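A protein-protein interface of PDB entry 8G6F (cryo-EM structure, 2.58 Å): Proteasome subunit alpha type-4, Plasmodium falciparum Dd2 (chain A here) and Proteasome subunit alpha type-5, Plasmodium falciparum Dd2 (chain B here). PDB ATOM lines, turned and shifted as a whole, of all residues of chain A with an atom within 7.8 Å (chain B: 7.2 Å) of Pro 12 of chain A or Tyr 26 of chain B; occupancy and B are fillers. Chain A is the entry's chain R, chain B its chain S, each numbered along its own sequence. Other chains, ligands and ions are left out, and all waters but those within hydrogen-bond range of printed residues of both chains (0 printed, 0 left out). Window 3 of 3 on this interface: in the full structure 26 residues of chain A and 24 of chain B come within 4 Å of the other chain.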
ATOM      1  N   VAL A   9      -8.625  19.110 -22.504  1.00  0.00           N
ATOM      2  CA  VAL A   9      -7.890  19.059 -21.250  1.00  0.00           C
ATOM      3  C   VAL A   9      -6.772  18.037 -21.389  1.00  0.00           C
ATOM      4  O   VAL A   9      -6.693  17.296 -22.368  1.00  0.00           O
ATOM      5  CB  VAL A   9      -8.797  18.706 -20.053  1.00  0.00           C
ATOM      6  CG1 VAL A   9      -9.774  19.829 -19.787  1.00  0.00           C
ATOM      7  CG2 VAL A   9      -9.533  17.406 -20.304  1.00  0.00           C
ATOM      8  N   PHE A  10      -5.900  18.005 -20.388  1.00  0.00           N
ATOM      9  CA  PHE A  10      -4.802  17.052 -20.373  1.00  0.00           C
ATOM     10  C   PHE A  10      -5.267  15.718 -19.809  1.00  0.00           C
ATOM     11  O   PHE A  10      -5.979  15.664 -18.804  1.00  0.00           O
ATOM     12  CB  PHE A  10      -3.635  17.583 -19.540  1.00  0.00           C
ATOM     13  CG  PHE A  10      -2.685  18.444 -20.313  1.00  0.00           C
ATOM     14  CD1 PHE A  10      -1.851  17.893 -21.267  1.00  0.00           C
ATOM     15  CD2 PHE A  10      -2.629  19.807 -20.090  1.00  0.00           C
ATOM     16  CE1 PHE A  10      -0.981  18.681 -21.979  1.00  0.00           C
ATOM     17  CE2 PHE A  10      -1.759  20.600 -20.801  1.00  0.00           C
ATOM     18  CZ  PHE A  10      -0.934  20.036 -21.748  1.00  0.00           C
ATOM     19  N   SER A  11      -4.876  14.647 -20.478  1.00  0.00           N
ATOM     20  CA  SER A  11      -5.073  13.305 -19.965  1.00  0.00           C
ATOM     21  C   SER A  11      -3.986  12.984 -18.946  1.00  0.00           C
ATOM     22  O   SER A  11      -2.939  13.631 -18.923  1.00  0.00           O
ATOM     23  CB  SER A  11      -5.048  12.300 -21.111  1.00  0.00           C
ATOM     24  OG  SER A  11      -4.484  11.066 -20.708  1.00  0.00           O
ATOM     25  N   PRO A  12      -4.205  11.984 -18.092  1.00  0.00           N
ATOM     26  CA  PRO A  12      -3.189  11.667 -17.077  1.00  0.00           C
ATOM     27  C   PRO A  12      -1.806  11.432 -17.654  1.00  0.00           C
ATOM     28  O   PRO A  12      -0.808  11.730 -16.988  1.00  0.00           O
ATOM     29  CB  PRO A  12      -3.747  10.403 -16.416  1.00  0.00           C
ATOM     30  CG  PRO A  12      -5.207  10.508 -16.594  1.00  0.00           C
ATOM     31  CD  PRO A  12      -5.422  11.174 -17.917  1.00  0.00           C
ATOM     32  N   ASP A  13      -1.713  10.913 -18.873  1.00  0.00           N
ATOM     33  CA  ASP A  13      -0.431  10.617 -19.495  1.00  0.00           C
ATOM     34  C   ASP A  13       0.185  11.819 -20.200  1.00  0.00           C
ATOM     35  O   ASP A  13       1.302  11.707 -20.711  1.00  0.00           O
ATOM     36  CB  ASP A  13      -0.598   9.468 -20.486  1.00  0.00           C
ATOM     37  CG  ASP A  13      -1.472   8.358 -19.940  1.00  0.00           C
ATOM     38  OD1 ASP A  13      -1.610   8.271 -18.702  1.00  0.00           O
ATOM     39  OD2 ASP A  13      -2.023   7.577 -20.743  1.00  0.00           O
ATOM     40  N   GLY A  14      -0.503  12.955 -20.238  1.00  0.00           N
ATOM     41  CA  GLY A  14       0.020  14.137 -20.888  1.00  0.00           C
ATOM     42  C   GLY A  14      -0.461  14.356 -22.302  1.00  0.00           C
ATOM     43  O   GLY A  14       0.190  15.092 -23.050  1.00  0.00           O
ATOM     44  N   HIS A  15      -1.576  13.748 -22.693  1.00  0.00           N
ATOM     45  CA  HIS A  15      -2.109  13.862 -24.041  1.00  0.00           C
ATOM     46  C   HIS A  15      -3.364  14.721 -24.047  1.00  0.00           C
ATOM     47  O   HIS A  15      -3.999  14.944 -23.016  1.00  0.00           O
ATOM     48  CB  HIS A  15      -2.432  12.481 -24.621  1.00  0.00           C
ATOM     49  CG  HIS A  15      -1.252  11.566 -24.686  1.00  0.00           C
ATOM     50  ND1 HIS A  15      -1.004  10.603 -23.733  1.00  0.00           N
ATOM     51  CD2 HIS A  15      -0.248  11.468 -25.589  1.00  0.00           C
ATOM     52  CE1 HIS A  15       0.101   9.952 -24.046  1.00  0.00           C
ATOM     53  NE2 HIS A  15       0.579  10.457 -25.167  1.00  0.00           N
ATOM     54  N   LEU A  17      -6.750  14.325 -25.594  1.00  0.00           N
ATOM     55  CA  LEU A  17      -7.590  13.336 -26.255  1.00  0.00           C
ATOM     56  C   LEU A  17      -8.500  13.973 -27.293  1.00  0.00           C
ATOM     57  O   LEU A  17      -8.801  13.350 -28.314  1.00  0.00           O
ATOM     58  CB  LEU A  17      -8.413  12.575 -25.219  1.00  0.00           C
ATOM     59  CG  LEU A  17      -7.623  11.698 -24.245  1.00  0.00           C
ATOM     60  CD1 LEU A  17      -8.564  10.827 -23.441  1.00  0.00           C
ATOM     61  CD2 LEU A  17      -6.597  10.840 -24.964  1.00  0.00           C
ATOM     62  N   ARG B  10     -12.883  15.872 -13.194  1.00  0.00           N
ATOM     63  CA  ARG B  10     -12.475  16.997 -12.371  1.00  0.00           C
ATOM     64  C   ARG B  10     -12.367  18.260 -13.209  1.00  0.00           C
ATOM     65  O   ARG B  10     -12.170  18.210 -14.425  1.00  0.00           O
ATOM     66  CB  ARG B  10     -11.129  16.713 -11.704  1.00  0.00           C
ATOM     67  CG  ARG B  10     -10.923  15.270 -11.301  1.00  0.00           C
ATOM     68  CD  ARG B  10      -9.939  15.170 -10.157  1.00  0.00           C
ATOM     69  NE  ARG B  10      -9.474  13.809  -9.929  1.00  0.00           N
ATOM     70  CZ  ARG B  10      -8.654  13.151 -10.736  1.00  0.00           C
ATOM     71  NH1 ARG B  10      -8.201  13.694 -11.854  1.00  0.00           N
ATOM     72  NH2 ARG B  10      -8.278  11.917 -10.414  1.00  0.00           N
ATOM     73  N   LEU B  21      -1.994  20.408  -8.498  1.00  0.00           N
ATOM     74  CA  LEU B  21      -3.021  20.560  -9.520  1.00  0.00           C
ATOM     75  C   LEU B  21      -2.872  19.451 -10.555  1.00  0.00           C
ATOM     76  O   LEU B  21      -1.800  19.287 -11.152  1.00  0.00           O
ATOM     77  CB  LEU B  21      -2.927  21.935 -10.176  1.00  0.00           C
ATOM     78  CG  LEU B  21      -3.109  23.122  -9.230  1.00  0.00           C
ATOM     79  CD1 LEU B  21      -2.633  24.405  -9.877  1.00  0.00           C
ATOM     80  CD2 LEU B  21      -4.556  23.251  -8.812  1.00  0.00           C
ATOM     81  N   PHE B  22      -3.956  18.704 -10.773  1.00  0.00           N
ATOM     82  CA  PHE B  22      -3.908  17.551 -11.665  1.00  0.00           C
ATOM     83  C   PHE B  22      -3.482  17.953 -13.068  1.00  0.00           C
ATOM     84  O   PHE B  22      -2.688  17.256 -13.710  1.00  0.00           O
ATOM     85  CB  PHE B  22      -5.276  16.874 -11.715  1.00  0.00           C
ATOM     86  CG  PHE B  22      -5.658  16.172 -10.448  1.00  0.00           C
ATOM     87  CD1 PHE B  22      -5.009  15.018 -10.057  1.00  0.00           C
ATOM     88  CD2 PHE B  22      -6.679  16.659  -9.657  1.00  0.00           C
ATOM     89  CE1 PHE B  22      -5.368  14.369  -8.898  1.00  0.00           C
ATOM     90  CE2 PHE B  22      -7.040  16.014  -8.498  1.00  0.00           C
ATOM     91  CZ  PHE B  22      -6.384  14.867  -8.120  1.00  0.00           C
ATOM     92  N   GLN B  23      -4.018  19.064 -13.571  1.00  0.00           N
ATOM     93  CA  GLN B  23      -3.681  19.498 -14.921  1.00  0.00           C
ATOM     94  C   GLN B  23      -2.205  19.844 -15.031  1.00  0.00           C
ATOM     95  O   GLN B  23      -1.567  19.557 -16.048  1.00  0.00           O
ATOM     96  CB  GLN B  23      -4.545  20.691 -15.320  1.00  0.00           C
ATOM     97  CG  GLN B  23      -5.961  20.315 -15.706  1.00  0.00           C
ATOM     98  CD  GLN B  23      -6.012  19.407 -16.913  1.00  0.00           C
ATOM     99  OE1 GLN B  23      -5.914  19.862 -18.049  1.00  0.00           O
ATOM    100  NE2 GLN B  23      -6.160  18.114 -16.673  1.00  0.00           N
ATOM    101  N   VAL B  24      -1.644  20.470 -13.997  1.00  0.00           N
ATOM    102  CA  VAL B  24      -0.221  20.783 -14.018  1.00  0.00           C
ATOM    103  C   VAL B  24       0.606  19.505 -14.006  1.00  0.00           C
ATOM    104  O   VAL B  24       1.615  19.399 -14.712  1.00  0.00           O
ATOM    105  CB  VAL B  24       0.141  21.706 -12.842  1.00  0.00           C
ATOM    106  CG1 VAL B  24       1.641  21.734 -12.634  1.00  0.00           C
ATOM    107  CG2 VAL B  24      -0.385  23.102 -13.099  1.00  0.00           C
ATOM    108  N   GLU B  25       0.201  18.514 -13.212  1.00  0.00           N
ATOM    109  CA  GLU B  25       0.936  17.253 -13.204  1.00  0.00           C
ATOM    110  C   GLU B  25       0.889  16.584 -14.572  1.00  0.00           C
ATOM    111  O   GLU B  25       1.893  16.037 -15.049  1.00  0.00           O
ATOM    112  CB  GLU B  25       0.372  16.326 -12.131  1.00  0.00           C
ATOM    113  CG  GLU B  25       0.391  16.918 -10.736  1.00  0.00           C
ATOM    114  CD  GLU B  25       1.792  17.201 -10.242  1.00  0.00           C
ATOM    115  OE1 GLU B  25       2.545  16.236 -10.005  1.00  0.00           O
ATOM    116  OE2 GLU B  25       2.144  18.389 -10.093  1.00  0.00           O
ATOM    117  N   TYR B  26      -0.270  16.625 -15.225  1.00  0.00           N
ATOM    118  CA  TYR B  26      -0.401  15.996 -16.533  1.00  0.00           C
ATOM    119  C   TYR B  26       0.399  16.745 -17.593  1.00  0.00           C
ATOM    120  O   TYR B  26       0.991  16.129 -18.488  1.00  0.00           O
ATOM    121  CB  TYR B  26      -1.876  15.911 -16.912  1.00  0.00           C
ATOM    122  CG  TYR B  26      -2.730  15.175 -15.900  1.00  0.00           C
ATOM    123  CD1 TYR B  26      -2.160  14.345 -14.945  1.00  0.00           C
ATOM    124  CD2 TYR B  26      -4.109  15.315 -15.899  1.00  0.00           C
ATOM    125  CE1 TYR B  26      -2.940  13.677 -14.027  1.00  0.00           C
ATOM    126  CE2 TYR B  26      -4.894  14.651 -14.986  1.00  0.00           C
ATOM    127  CZ  TYR B  26      -4.307  13.834 -14.053  1.00  0.00           C
ATOM    128  OH  TYR B  26      -5.090  13.170 -13.138  1.00  0.00           O
ATOM    129  N   ALA B  27       0.446  18.074 -17.508  1.00  0.00           N
ATOM    130  CA  ALA B  27       1.297  18.837 -18.415  1.00  0.00           C
ATOM    131  C   ALA B  27       2.771  18.522 -18.179  1.00  0.00           C
ATOM    132  O   ALA B  27       3.574  18.491 -19.124  1.00  0.00           O
ATOM    133  CB  ALA B  27       1.026  20.330 -18.247  1.00  0.00           C
ATOM    134  N   LEU B  28       3.152  18.308 -16.919  1.00  0.00           N
ATOM    135  CA  LEU B  28       4.517  17.889 -16.629  1.00  0.00           C
ATOM    136  C   LEU B  28       4.813  16.550 -17.282  1.00  0.00           C
ATOM    137  O   LEU B  28       5.908  16.334 -17.813  1.00  0.00           O
ATOM    138  CB  LEU B  28       4.737  17.807 -15.119  1.00  0.00           C
ATOM    139  CG  LEU B  28       4.886  19.138 -14.383  1.00  0.00           C
ATOM    140  CD1 LEU B  28       4.951  18.903 -12.887  1.00  0.00           C
ATOM    141  CD2 LEU B  28       6.110  19.887 -14.857  1.00  0.00           C
ATOM    142  N   GLY B  29       3.852  15.635 -17.246  1.00  0.00           N
ATOM    143  CA  GLY B  29       4.002  14.405 -18.002  1.00  0.00           C
ATOM    144  C   GLY B  29       4.142  14.655 -19.491  1.00  0.00           C
ATOM    145  O   GLY B  29       4.867  13.936 -20.182  1.00  0.00           O
ATOM    146  N   ALA B  30       3.447  15.669 -20.004  1.00  0.00           N
ATOM    147  CA  ALA B  30       3.496  15.958 -21.435  1.00  0.00           C
ATOM    148  C   ALA B  30       4.871  16.452 -21.870  1.00  0.00           C
ATOM    149  O   ALA B  30       5.347  16.095 -22.953  1.00  0.00           O
ATOM    150  CB  ALA B  30       2.432  16.992 -21.798  1.00  0.00           C
ATOM    151  N   ILE B  31       5.519  17.284 -21.057  1.00  0.00           N
ATOM    152  CA  ILE B  31       6.754  17.939 -21.497  1.00  0.00           C
ATOM    153  C   ILE B  31       7.904  16.948 -21.649  1.00  0.00           C
ATOM    154  O   ILE B  31       8.986  17.313 -22.118  1.00  0.00           O
ATOM    155  CB  ILE B  31       7.176  19.070 -20.541  1.00  0.00           C
ATOM    156  CG1 ILE B  31       7.398  18.537 -19.126  1.00  0.00           C
ATOM    157  CG2 ILE B  31       6.146  20.166 -20.542  1.00  0.00           C
ATOM    158  CD1 ILE B  31       8.214  19.460 -18.252  1.00  0.00           C
ATOM    159  N   PRO B 138      -3.200  24.182 -18.893  1.00  0.00           N
ATOM    160  CA  PRO B 138      -1.758  24.440 -18.959  1.00  0.00           C
ATOM    161  C   PRO B 138      -1.239  24.322 -20.383  1.00  0.00           C
ATOM    162  O   PRO B 138      -1.928  23.875 -21.299  1.00  0.00           O
ATOM    163  CB  PRO B 138      -1.162  23.361 -18.051  1.00  0.00           C
ATOM    164  CG  PRO B 138      -2.258  22.972 -17.151  1.00  0.00           C
ATOM    165  CD  PRO B 138      -3.529  23.137 -17.912  1.00  0.00           C
ATOM    166  N   GLY B 140       1.862  22.707 -21.203  1.00  0.00           N
ATOM    167  CA  GLY B 140       2.576  21.479 -21.482  1.00  0.00           C
ATOM    168  C   GLY B 140       3.798  21.731 -22.336  1.00  0.00           C
ATOM    169  O   GLY B 140       4.044  21.026 -23.319  1.00  0.00           O
ATOM    170  N   PRO B 160       5.701  23.752 -17.174  1.00  0.00           N
ATOM    171  CA  PRO B 160       4.255  24.024 -17.145  1.00  0.00           C
ATOM    172  C   PRO B 160       3.735  24.449 -15.787  1.00  0.00           C
ATOM    173  O   PRO B 160       2.727  25.162 -15.721  1.00  0.00           O
ATOM    174  CB  PRO B 160       3.643  22.687 -17.579  1.00  0.00           C
ATOM    175  CG  PRO B 160       4.696  22.009 -18.341  1.00  0.00           C
ATOM    176  CD  PRO B 160       6.003  22.439 -17.765  1.00  0.00           C
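Of the printed residues of chain B, Val 9 of chain A touches Gln 23.
Of the printed residues of chain B, Pro 12 of chain A touches Tyr 26 (3.6 Å).
Tyr 26 of chain B touches just these residues of chain A: Phe 10, Ser 11, Pro 12 and Gly 14.
Of chain A, only Phe 10 comes within 4 Å of Ala 27 of chain B.
Gly 29 of chain B touches none of the printed residues of chain A.
Of the printed residues of chain A, Gly 140 of chain B touches Phe 10 (3.8 Å).
The nearest residue of chain B that does not touch Pro 12 of chain A is Glu 25 of chain B (5.4 Å).
NH1 of Arg 10 of chain B sits at hydrogen-bond distance from OH of Tyr 26 of chain B (3.4 Å).
OG of Ser 11 of chain A lies close to N of Asp 13 of chain A (3.3 Å).
The backbone NH of Phe 10 of chain A is in hydrogen-bond range of the side-chain amide oxygen of Gln 23 of chain B.
Hydrophobic or aromatic side chains of chain A that line the printed part of chain B: Val 9 and Phe 10.
Among the printed residues, 11 pairs touch across the chains.
Among the printed residues, no Asp or Glu carboxylate lies within 4 Å of a Lys or Arg side-chain nitrogen of the other chain.
Among the printed residues, merely in contact across the chains: Gly 14 of chain A with Ala 30 of chain B, Ser 11 of chain A with Tyr 26 of chain B, Gly 14 of chain A with Tyr 26 of chain B, Phe 10 of chain A with Pro 138 of chain B, Phe 10 of chain A with Tyr 26 of chain B, Pro 12 of chain A with Tyr 26 of chain B, Val 9 of chain A with Gln 23 of chain B, Phe 10 of chain A with Ala 27 of chain B, Phe 10 of chain A with Gly 140 of chain B and Phe 10 of chain A with Ala 30 of chain B.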
